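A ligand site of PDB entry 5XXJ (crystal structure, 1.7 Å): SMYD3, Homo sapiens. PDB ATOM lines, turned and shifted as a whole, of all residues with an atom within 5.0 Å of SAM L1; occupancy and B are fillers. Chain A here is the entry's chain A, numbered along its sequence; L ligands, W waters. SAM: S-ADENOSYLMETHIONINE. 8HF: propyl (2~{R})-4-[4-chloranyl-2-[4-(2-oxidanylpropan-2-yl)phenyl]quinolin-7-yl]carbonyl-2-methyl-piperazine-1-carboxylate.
SD of SAM L1 sits close to OD1 of Asn 179 (3.6 Å). O of Ser 200 sits close to SD of SAM L1 (3.4 Å). OH of Tyr 237 sits close to SD of SAM L1. Merely in contact with SAM L1: Gly 13, Glu 128, Cys 178, Leu 201, Leu 202 and Phe 257. Hydrophobic or aromatic side chains that line SAM L1: Tyr 122, His 204, Tyr 237, Tyr 255 and Phe 257. Of the 22 residues printed, 16 come within 4 Å of SAM L1. The nearest printed residue that does not touch SAM L1 is Asn 11 (4.6 Å).
O of Tyr 255 sits at hydrogen-bond distance from ND2 of Asn 130, 3.5 Å away. The side-chain amide nitrogen of Asn 14 sits at hydrogen-bond distance from the side-chain hydroxyl of Tyr 122, at 3.0 Å. The backbone carbonyl oxygen (O) of Asp 126 is in hydrogen-bond range of the side-chain hydroxyl (OH) of Tyr 122, at 3.2 Å. The backbone carbonyl oxygen (O) of Arg 12 is in hydrogen-bond range of the side-chain amide nitrogen (ND2) of Asn 203, at 3.4 Å. The backbone NH of Tyr 237 is in hydrogen-bond range of a ring nitrogen (ND1) of His 204. O of Glu 128 is in hydrogen-bond range of ND2 of Asn 179. The side-chain amide nitrogen (ND2) of Asn 179 is in hydrogen-bond range of the side-chain sulfur (SG) of Cys 178, 3.5 Å away. The backbone carbonyl oxygen (O) of Leu 202 lies within hydrogen-bond range of the side-chain hydroxyl (OH) of Tyr 237 (2.6 Å).
The backbone carbonyl oxygen of Tyr 255 is in hydrogen-bond range of an oxygen (O3') of SAM L1 (2.6 Å). The side-chain hydroxyl of Tyr 122 sits at hydrogen-bond distance from an oxygen (OXT) of SAM L1 (2.7 Å). The backbone carbonyl oxygen (O) of Arg 12 lies within hydrogen-bond range of a nitrogen (N) of SAM L1 (2.8 Å). An oxygen (O) of SAM L1 is in hydrogen-bond range of the backbone NH (N) of Asn 14. The backbone carbonyl oxygen (O) of Asn 14 lies within hydrogen-bond range of a nitrogen (N) of SAM L1 (2.9 Å). The side-chain amide nitrogen (ND2) of Asn 130 sits at hydrogen-bond distance from an oxygen (O3') of SAM L1 (2.8 Å). A nitrogen (N7) of SAM L1 lies within hydrogen-bond range of the backbone NH (N) of His 204, at 3.0 Å. The backbone carbonyl oxygen (O) of His 204 sits at hydrogen-bond distance from a nitrogen (N6) of SAM L1. The side-chain amide oxygen of Asn 203 sits at hydrogen-bond distance from a nitrogen (N) of SAM L1 (2.9 Å). The side-chain hydroxyl (OH) of Tyr 255 sits at hydrogen-bond distance from an oxygen (OBG) of 8HF L2 (2.7 Å).
Water W1 lies within hydrogen-bond range of an oxygen (O) of SAM L1 (2.7 Å) and the side-chain carboxylate of Glu 128 (3.0 Å). Water W4 lies within hydrogen-bond range of the side-chain amide oxygen (OD1) of Asn 179, the backbone NH (N) of Glu 128 and an oxygen (OXT) of SAM L1. Water W6 lies within hydrogen-bond range of the backbone carbonyl oxygen (O) of Cys 256 (2.7 Å), an oxygen (O2') of SAM L1 (2.8 Å) and the side-chain amide oxygen (OD1) of Asn 130 (3.1 Å). Water W3 bridges a nitrogen (N) of SAM L1 and the side-chain carboxylate (OE1) of Glu 128. Water W8 lies within hydrogen-bond range of the backbone carbonyl oxygen of Glu 258 (2.9 Å) and a nitrogen (N1) of SAM L1 (3.1 Å).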
ATOM      1  N   ASN A  11      20.294  37.584   8.594  1.00  0.00           N
ATOM      2  CA  ASN A  11      20.949  37.662   9.893  1.00  0.00           C
ATOM      3  C   ASN A  11      20.442  36.623  10.901  1.00  0.00           C
ATOM      4  O   ASN A  11      20.673  36.796  12.104  1.00  0.00           O
ATOM      5  CB  ASN A  11      20.808  39.088  10.498  1.00  0.00           C
ATOM      6  CG  ASN A  11      19.366  39.517  10.740  1.00  0.00           C
ATOM      7  OD1 ASN A  11      18.451  38.696  10.885  1.00  0.00           O
ATOM      8  ND2 ASN A  11      19.154  40.817  10.801  1.00  0.00           N
ATOM      9  N   ARG A  12      19.775  35.568  10.462  1.00  0.00           N
ATOM     10  CA  ARG A  12      19.415  34.507  11.405  1.00  0.00           C
ATOM     11  C   ARG A  12      19.678  33.153  10.779  1.00  0.00           C
ATOM     12  O   ARG A  12      18.900  32.201  10.956  1.00  0.00           O
ATOM     13  CB  ARG A  12      17.966  34.613  11.866  1.00  0.00           C
ATOM     14  CG  ARG A  12      17.007  35.159  10.861  1.00  0.00           C
ATOM     15  CD  ARG A  12      15.856  35.787  11.588  1.00  0.00           C
ATOM     16  NE  ARG A  12      14.633  35.851  10.807  1.00  0.00           N
ATOM     17  CZ  ARG A  12      13.549  36.505  11.217  1.00  0.00           C
ATOM     18  NH1 ARG A  12      13.563  37.127  12.395  1.00  0.00           N
ATOM     19  NH2 ARG A  12      12.453  36.530  10.461  1.00  0.00           N
ATOM     20  N   GLY A  13      20.790  33.039  10.058  1.00  0.00           N
ATOM     21  CA  GLY A  13      21.184  31.727   9.579  1.00  0.00           C
ATOM     22  C   GLY A  13      20.301  31.259   8.440  1.00  0.00           C
ATOM     23  O   GLY A  13      19.792  32.053   7.641  1.00  0.00           O
ATOM     24  N   ASN A  14      20.118  29.941   8.349  1.00  0.00           N
ATOM     25  CA  ASN A  14      19.195  29.409   7.359  1.00  0.00           C
ATOM     26  C   ASN A  14      17.763  29.503   7.877  1.00  0.00           C
ATOM     27  O   ASN A  14      17.520  29.572   9.080  1.00  0.00           O
ATOM     28  CB  ASN A  14      19.549  27.952   7.045  1.00  0.00           C
ATOM     29  CG  ASN A  14      20.920  27.855   6.407  1.00  0.00           C
ATOM     30  OD1 ASN A  14      21.240  28.626   5.497  1.00  0.00           O
ATOM     31  ND2 ASN A  14      21.743  26.945   6.906  1.00  0.00           N
ATOM     32  N   TYR A 122      16.992  19.364   5.355  1.00  0.00           N
ATOM     33  CA  TYR A 122      18.034  19.759   6.296  1.00  0.00           C
ATOM     34  C   TYR A 122      18.326  18.537   7.131  1.00  0.00           C
ATOM     35  O   TYR A 122      17.394  17.870   7.575  1.00  0.00           O
ATOM     36  CB  TYR A 122      17.529  20.887   7.210  1.00  0.00           C
ATOM     37  CG  TYR A 122      18.513  21.946   7.700  1.00  0.00           C
ATOM     38  CD1 TYR A 122      19.432  22.550   6.857  1.00  0.00           C
ATOM     39  CD2 TYR A 122      18.425  22.397   9.013  1.00  0.00           C
ATOM     40  CE1 TYR A 122      20.265  23.570   7.317  1.00  0.00           C
ATOM     41  CE2 TYR A 122      19.262  23.401   9.489  1.00  0.00           C
ATOM     42  CZ  TYR A 122      20.182  23.980   8.632  1.00  0.00           C
ATOM     43  OH  TYR A 122      20.989  24.982   9.110  1.00  0.00           O
ATOM     44  N   ASP A 126      23.554  19.290   9.332  1.00  0.00           N
ATOM     45  CA  ASP A 126      23.392  20.699   8.975  1.00  0.00           C
ATOM     46  C   ASP A 126      22.977  21.570  10.145  1.00  0.00           C
ATOM     47  O   ASP A 126      23.069  22.791  10.031  1.00  0.00           O
ATOM     48  CB  ASP A 126      22.322  20.870   7.898  1.00  0.00           C
ATOM     49  CG  ASP A 126      22.646  20.178   6.593  1.00  0.00           C
ATOM     50  OD1 ASP A 126      23.814  20.181   6.157  1.00  0.00           O
ATOM     51  OD2 ASP A 126      21.697  19.661   5.969  1.00  0.00           O
ATOM     52  N   LEU A 127      22.486  20.970  11.232  1.00  0.00           N
ATOM     53  CA  LEU A 127      21.825  21.749  12.278  1.00  0.00           C
ATOM     54  C   LEU A 127      22.766  22.773  12.908  1.00  0.00           C
ATOM     55  O   LEU A 127      23.965  22.548  13.080  1.00  0.00           O
ATOM     56  CB  LEU A 127      21.304  20.829  13.365  1.00  0.00           C
ATOM     57  CG  LEU A 127      20.148  19.903  13.001  1.00  0.00           C
ATOM     58  CD1 LEU A 127      19.786  19.036  14.228  1.00  0.00           C
ATOM     59  CD2 LEU A 127      18.924  20.667  12.501  1.00  0.00           C
ATOM     60  N   GLU A 128      22.169  23.894  13.294  1.00  0.00           N
ATOM     61  CA  GLU A 128      22.910  24.951  13.980  1.00  0.00           C
ATOM     62  C   GLU A 128      23.342  24.488  15.362  1.00  0.00           C
ATOM     63  O   GLU A 128      22.544  23.900  16.108  1.00  0.00           O
ATOM     64  CB  GLU A 128      22.012  26.188  14.085  1.00  0.00           C
ATOM     65  CG  GLU A 128      22.641  27.296  14.909  1.00  0.00           C
ATOM     66  CD  GLU A 128      23.815  27.902  14.206  1.00  0.00           C
ATOM     67  OE1 GLU A 128      23.586  28.669  13.239  1.00  0.00           O
ATOM     68  OE2 GLU A 128      24.973  27.604  14.603  1.00  0.00           O
ATOM     69  N   ASN A 130      25.529  26.807  17.336  1.00  0.00           N
ATOM     70  CA  ASN A 130      25.795  28.047  18.090  1.00  0.00           C
ATOM     71  C   ASN A 130      27.033  27.934  18.980  1.00  0.00           C
ATOM     72  O   ASN A 130      27.131  28.599  20.023  1.00  0.00           O
ATOM     73  CB  ASN A 130      24.574  28.453  18.914  1.00  0.00           C
ATOM     74  CG  ASN A 130      23.504  29.055  18.066  1.00  0.00           C
ATOM     75  OD1 ASN A 130      23.784  29.878  17.205  1.00  0.00           O
ATOM     76  ND2 ASN A 130      22.265  28.630  18.295  1.00  0.00           N
ATOM     77  N   CYS A 178      19.581  23.373  20.913  1.00  0.00           N
ATOM     78  CA  CYS A 178      18.789  24.388  20.230  1.00  0.00           C
ATOM     79  C   CYS A 178      17.935  23.828  19.088  1.00  0.00           C
ATOM     80  O   CYS A 178      17.341  24.616  18.338  1.00  0.00           O
ATOM     81  CB  CYS A 178      19.691  25.508  19.728  1.00  0.00           C
ATOM     82  SG  CYS A 178      20.913  25.023  18.518  1.00  0.00           S
ATOM     83  N   ASN A 179      17.819  22.507  18.960  1.00  0.00           N
ATOM     84  CA  ASN A 179      16.958  21.931  17.939  1.00  0.00           C
ATOM     85  C   ASN A 179      16.023  20.837  18.436  1.00  0.00           C
ATOM     86  O   ASN A 179      15.337  20.219  17.616  1.00  0.00           O
ATOM     87  CB  ASN A 179      17.809  21.375  16.788  1.00  0.00           C
ATOM     88  CG  ASN A 179      18.551  22.440  16.040  1.00  0.00           C
ATOM     89  OD1 ASN A 179      17.966  23.151  15.210  1.00  0.00           O
ATOM     90  ND2 ASN A 179      19.846  22.571  16.302  1.00  0.00           N
ATOM     91  N   SER A 200      13.499  22.029  11.751  1.00  0.00           N
ATOM     92  CA  SER A 200      14.435  22.879  12.469  1.00  0.00           C
ATOM     93  C   SER A 200      14.894  24.074  11.646  1.00  0.00           C
ATOM     94  O   SER A 200      15.599  24.931  12.177  1.00  0.00           O
ATOM     95  CB  SER A 200      15.656  22.087  12.915  1.00  0.00           C
ATOM     96  OG  SER A 200      15.378  21.366  14.101  1.00  0.00           O
ATOM     97  N   LEU A 201      14.540  24.146  10.363  1.00  0.00           N
ATOM     98  CA  LEU A 201      14.821  25.352   9.579  1.00  0.00           C
ATOM     99  C   LEU A 201      13.991  26.550  10.040  1.00  0.00           C
ATOM    100  O   LEU A 201      14.355  27.693   9.734  1.00  0.00           O
ATOM    101  CB  LEU A 201      14.558  25.109   8.096  1.00  0.00           C
ATOM    102  CG  LEU A 201      15.710  24.392   7.387  1.00  0.00           C
ATOM    103  CD1 LEU A 201      15.290  23.971   5.971  1.00  0.00           C
ATOM    104  CD2 LEU A 201      16.923  25.293   7.376  1.00  0.00           C
ATOM    105  N   LEU A 202      12.890  26.319  10.734  1.00  0.00           N
ATOM    106  CA  LEU A 202      11.997  27.428  11.069  1.00  0.00           C
ATOM    107  C   LEU A 202      12.649  28.314  12.120  1.00  0.00           C
ATOM    108  O   LEU A 202      12.992  27.854  13.213  1.00  0.00           O
ATOM    109  CB  LEU A 202      10.665  26.912  11.585  1.00  0.00           C
ATOM    110  CG  LEU A 202       9.809  26.226  10.515  1.00  0.00           C
ATOM    111  CD1 LEU A 202       8.877  25.250  11.152  1.00  0.00           C
ATOM    112  CD2 LEU A 202       9.032  27.262   9.688  1.00  0.00           C
ATOM    113  N   ASN A 203      12.796  29.596  11.805  1.00  0.00           N
ATOM    114  CA  ASN A 203      13.229  30.531  12.835  1.00  0.00           C
ATOM    115  C   ASN A 203      12.040  30.965  13.700  1.00  0.00           C
ATOM    116  O   ASN A 203      10.885  30.699  13.388  1.00  0.00           O
ATOM    117  CB  ASN A 203      13.910  31.734  12.215  1.00  0.00           C
ATOM    118  CG  ASN A 203      15.275  31.398  11.696  1.00  0.00           C
ATOM    119  OD1 ASN A 203      16.061  30.782  12.409  1.00  0.00           O
ATOM    120  ND2 ASN A 203      15.552  31.749  10.439  1.00  0.00           N
ATOM    121  N   HIS A 204      12.373  31.645  14.797  1.00  0.00           N
ATOM    122  CA  HIS A 204      11.429  32.020  15.844  1.00  0.00           C
ATOM    123  C   HIS A 204      10.829  33.390  15.613  1.00  0.00           C
ATOM    124  O   HIS A 204      11.515  34.319  15.197  1.00  0.00           O
ATOM    125  CB  HIS A 204      12.133  32.056  17.195  1.00  0.00           C
ATOM    126  CG  HIS A 204      11.341  32.753  18.266  1.00  0.00           C
ATOM    127  ND1 HIS A 204      10.398  32.107  19.019  1.00  0.00           N
ATOM    128  CD2 HIS A 204      11.337  34.043  18.685  1.00  0.00           C
ATOM    129  CE1 HIS A 204       9.854  32.949  19.880  1.00  0.00           C
ATOM    130  NE2 HIS A 204      10.405  34.140  19.683  1.00  0.00           N
ATOM    131  N   SER A 205       9.547  33.525  15.960  1.00  0.00           N
ATOM    132  CA  SER A 205       8.890  34.816  16.106  1.00  0.00           C
ATOM    133  C   SER A 205       7.971  34.776  17.305  1.00  0.00           C
ATOM    134  O   SER A 205       7.285  33.769  17.536  1.00  0.00           O
ATOM    135  CB  SER A 205       8.085  35.184  14.842  1.00  0.00           C
ATOM    136  OG  SER A 205       7.430  36.420  15.047  1.00  0.00           O
ATOM    137  N   TYR A 237       8.906  29.533  19.364  1.00  0.00           N
ATOM    138  CA  TYR A 237       9.566  28.466  20.103  1.00  0.00           C
ATOM    139  C   TYR A 237       9.063  28.344  21.544  1.00  0.00           C
ATOM    140  O   TYR A 237       9.366  27.346  22.211  1.00  0.00           O
ATOM    141  CB  TYR A 237      11.073  28.726  20.183  1.00  0.00           C
ATOM    142  CG  TYR A 237      11.868  28.698  18.888  1.00  0.00           C
ATOM    143  CD1 TYR A 237      11.276  28.470  17.653  1.00  0.00           C
ATOM    144  CD2 TYR A 237      13.254  28.906  18.919  1.00  0.00           C
ATOM    145  CE1 TYR A 237      12.042  28.443  16.475  1.00  0.00           C
ATOM    146  CE2 TYR A 237      14.022  28.873  17.753  1.00  0.00           C
ATOM    147  CZ  TYR A 237      13.411  28.649  16.539  1.00  0.00           C
ATOM    148  OH  TYR A 237      14.157  28.623  15.372  1.00  0.00           O
ATOM    149  N   TYR A 255      18.792  29.319  22.912  1.00  0.00           N
ATOM    150  CA  TYR A 255      18.902  29.549  21.474  1.00  0.00           C
ATOM    151  C   TYR A 255      19.944  30.585  21.084  1.00  0.00           C
ATOM    152  O   TYR A 255      20.125  30.833  19.877  1.00  0.00           O
ATOM    153  CB  TYR A 255      17.545  29.946  20.900  1.00  0.00           C
ATOM    154  CG  TYR A 255      16.533  28.835  21.102  1.00  0.00           C
ATOM    155  CD1 TYR A 255      16.569  27.676  20.313  1.00  0.00           C
ATOM    156  CD2 TYR A 255      15.574  28.913  22.119  1.00  0.00           C
ATOM    157  CE1 TYR A 255      15.648  26.646  20.504  1.00  0.00           C
ATOM    158  CE2 TYR A 255      14.663  27.897  22.315  1.00  0.00           C
ATOM    159  CZ  TYR A 255      14.704  26.777  21.514  1.00  0.00           C
ATOM    160  OH  TYR A 255      13.785  25.757  21.733  1.00  0.00           O
ATOM    161  N   CYS A 256      20.625  31.195  22.053  1.00  0.00           N
ATOM    162  CA  CYS A 256      21.706  32.159  21.789  1.00  0.00           C
ATOM    163  C   CYS A 256      21.312  33.247  20.804  1.00  0.00           C
ATOM    164  O   CYS A 256      22.068  33.586  19.888  1.00  0.00           O
ATOM    165  CB  CYS A 256      22.968  31.445  21.282  1.00  0.00           C
ATOM    166  SG  CYS A 256      23.736  30.306  22.426  1.00  0.00           S
ATOM    167  N   PHE A 257      20.130  33.833  20.968  1.00  0.00           N
ATOM    168  CA  PHE A 257      19.886  35.049  20.195  1.00  0.00           C
ATOM    169  C   PHE A 257      19.042  36.013  20.995  1.00  0.00           C
ATOM    170  O   PHE A 257      18.408  35.655  22.003  1.00  0.00           O
ATOM    171  CB  PHE A 257      19.242  34.790  18.816  1.00  0.00           C
ATOM    172  CG  PHE A 257      17.795  34.371  18.878  1.00  0.00           C
ATOM    173  CD1 PHE A 257      17.441  33.045  19.105  1.00  0.00           C
ATOM    174  CD2 PHE A 257      16.795  35.309  18.675  1.00  0.00           C
ATOM    175  CE1 PHE A 257      16.090  32.667  19.157  1.00  0.00           C
ATOM    176  CE2 PHE A 257      15.452  34.938  18.715  1.00  0.00           C
ATOM    177  CZ  PHE A 257      15.100  33.619  18.960  1.00  0.00           C
ATOM    178  N   GLU A 258      19.099  37.267  20.558  1.00  0.00           N
ATOM    179  CA  GLU A 258      18.328  38.373  21.107  1.00  0.00           C
ATOM    180  C   GLU A 258      17.211  38.709  20.137  1.00  0.00           C
ATOM    181  O   GLU A 258      17.446  38.829  18.936  1.00  0.00           O
ATOM    182  CB  GLU A 258      19.226  39.605  21.305  1.00  0.00           C
ATOM    183  CG  GLU A 258      20.688  39.276  21.682  1.00  0.00           C
ATOM    184  CD  GLU A 258      20.818  38.878  23.127  1.00  0.00           C
ATOM    185  OE1 GLU A 258      19.823  39.057  23.872  1.00  0.00           O
ATOM    186  OE2 GLU A 258      21.903  38.404  23.532  1.00  0.00           O
HETATM  187  N   SAM L   1      18.608  29.558  11.738  1.00  0.00           N
HETATM  188  CA  SAM L   1      18.707  28.141  12.059  1.00  0.00           C
HETATM  189  C   SAM L   1      19.738  27.451  11.180  1.00  0.00           C
HETATM  190  O   SAM L   1      20.492  28.131  10.481  1.00  0.00           O
HETATM  191  OXT SAM L   1      19.829  26.220  11.189  1.00  0.00           O
HETATM  192  CB  SAM L   1      17.336  27.470  11.922  1.00  0.00           C
HETATM  193  CG  SAM L   1      16.514  27.568  13.219  1.00  0.00           C
HETATM  194  SD  SAM L   1      17.254  26.635  14.594  1.00  0.00           S
HETATM  195  CE  SAM L   1      15.853  25.650  15.191  1.00  0.00           C
HETATM  196  C5' SAM L   1      17.313  27.868  15.920  1.00  0.00           C
HETATM  197  C4' SAM L   1      18.467  28.839  15.786  1.00  0.00           C
HETATM  198  O4' SAM L   1      18.174  29.779  14.757  1.00  0.00           O
HETATM  199  C3' SAM L   1      18.678  29.692  17.045  1.00  0.00           C
HETATM  200  O3' SAM L   1      19.480  29.078  18.031  1.00  0.00           O
HETATM  201  C2' SAM L   1      19.321  30.931  16.491  1.00  0.00           C
HETATM  202  O2' SAM L   1      20.650  30.656  16.080  1.00  0.00           O
HETATM  203  C1' SAM L   1      18.575  31.073  15.190  1.00  0.00           C
HETATM  204  N9  SAM L   1      17.327  31.867  15.302  1.00  0.00           N
HETATM  205  C8  SAM L   1      16.068  31.327  15.306  1.00  0.00           C
HETATM  206  N7  SAM L   1      15.185  32.347  15.353  1.00  0.00           N
HETATM  207  C5  SAM L   1      15.859  33.524  15.364  1.00  0.00           C
HETATM  208  C6  SAM L   1      15.462  34.851  15.417  1.00  0.00           C
HETATM  209  N6  SAM L   1      14.186  35.252  15.468  1.00  0.00           N
HETATM  210  N1  SAM L   1      16.439  35.812  15.424  1.00  0.00           N
HETATM  211  C2  SAM L   1      17.778  35.492  15.374  1.00  0.00           C
HETATM  212  N3  SAM L   1      18.183  34.188  15.323  1.00  0.00           N
HETATM  213  C4  SAM L   1      17.227  33.220  15.318  1.00  0.00           C
HETATM  214  CAA 8HF L   2       4.252  21.020  22.229  1.00  0.00           C
HETATM  215  CAB 8HF L   2       4.951  21.607  21.185  1.00  0.00           C
HETATM  216  CAC 8HF L   2       5.047  22.988  21.073  1.00  0.00           C
HETATM  217  CAD 8HF L   2       4.580  23.763  22.128  1.00  0.00           C
HETATM  218  CAE 8HF L   2       3.805  23.201  23.149  1.00  0.00           C
HETATM  219  CAF 8HF L   2       3.674  21.824  23.220  1.00  0.00           C
HETATM  220  CAH 8HF L   2       2.551  23.448  25.131  1.00  0.00           C
HETATM  221  CAI 8HF L   2       2.414  22.072  25.244  1.00  0.00           C
HETATM  222  CAJ 8HF L   2       2.974  21.250  24.270  1.00  0.00           C
HETATM  223  CAK 8HF L   2       2.009  24.281  26.099  1.00  0.00           C
HETATM  224  CAL 8HF L   2       2.380  25.618  26.173  1.00  0.00           C
HETATM  225  CAM 8HF L   2       1.840  26.446  27.154  1.00  0.00           C
HETATM  226  CAN 8HF L   2       0.930  25.946  28.089  1.00  0.00           C
HETATM  227  CAO 8HF L   2       0.560  24.599  28.019  1.00  0.00           C
HETATM  228  CAP 8HF L   2       1.122  23.767  27.048  1.00  0.00           C
HETATM  229  CAQ 8HF L   2       0.397  26.805  29.070  1.00  0.00           C
HETATM  230  CAR 8HF L   2      -0.689  27.637  28.392  1.00  0.00           C
HETATM  231  CAS 8HF L   2      -0.232  26.016  30.216  1.00  0.00           C
HETATM  232  CAV 8HF L   2       5.804  23.466  19.996  1.00  0.00           C
HETATM  233  CAY 8HF L   2       7.441  24.970  21.100  1.00  0.00           C
HETATM  234  CAZ 8HF L   2       8.833  24.232  20.971  1.00  0.00           C
HETATM  235  CBB 8HF L   2       8.687  24.331  18.540  1.00  0.00           C
HETATM  236  CBC 8HF L   2       7.349  25.021  18.765  1.00  0.00           C
HETATM  237  CBD 8HF L   2      10.845  24.696  19.605  1.00  0.00           C
HETATM  238  CBE 8HF L   2       8.727  22.701  21.047  1.00  0.00           C
HETATM  239  CBH 8HF L   2      12.815  25.242  18.616  1.00  0.00           C
HETATM  240  CBI 8HF L   2      13.650  23.995  18.371  1.00  0.00           C
HETATM  241  CBJ 8HF L   2      13.508  23.589  16.922  1.00  0.00           C
HETATM  242  NAG 8HF L   2       3.279  23.973  24.115  1.00  0.00           N
HETATM  243  NAW 8HF L   2       6.581  24.568  19.960  1.00  0.00           N
HETATM  244  NBA 8HF L   2       9.525  24.559  19.705  1.00  0.00           N
HETATM  245  OAT 8HF L   2       1.416  27.664  29.611  1.00  0.00           O
HETATM  246  OAX 8HF L   2       5.277  23.167  18.949  1.00  0.00           O
HETATM  247  OBF 8HF L   2      11.413  25.004  18.396  1.00  0.00           O
HETATM  248  OBG 8HF L   2      11.493  24.775  20.642  1.00  0.00           O
HETATM  249  O   HOH W   1      23.137  27.631  10.498  1.00  0.00           O
HETATM  250  O   HOH W   2      13.228  38.141  16.090  1.00  0.00           O
HETATM  251  O   HOH W   3      21.090  30.203  13.092  1.00  0.00           O
HETATM  252  O   HOH W   4      19.375  24.115  13.019  1.00  0.00           O
HETATM  253  O   HOH W   5      19.247  38.331  14.126  1.00  0.00           O
HETATM  254  O   HOH W   6      22.261  32.556  17.417  1.00  0.00           O
HETATM  255  O   HOH W   7      20.998  34.322  15.241  1.00  0.00           O
HETATM  256  O   HOH W   8      16.222  38.795  16.282  1.00  0.00           O
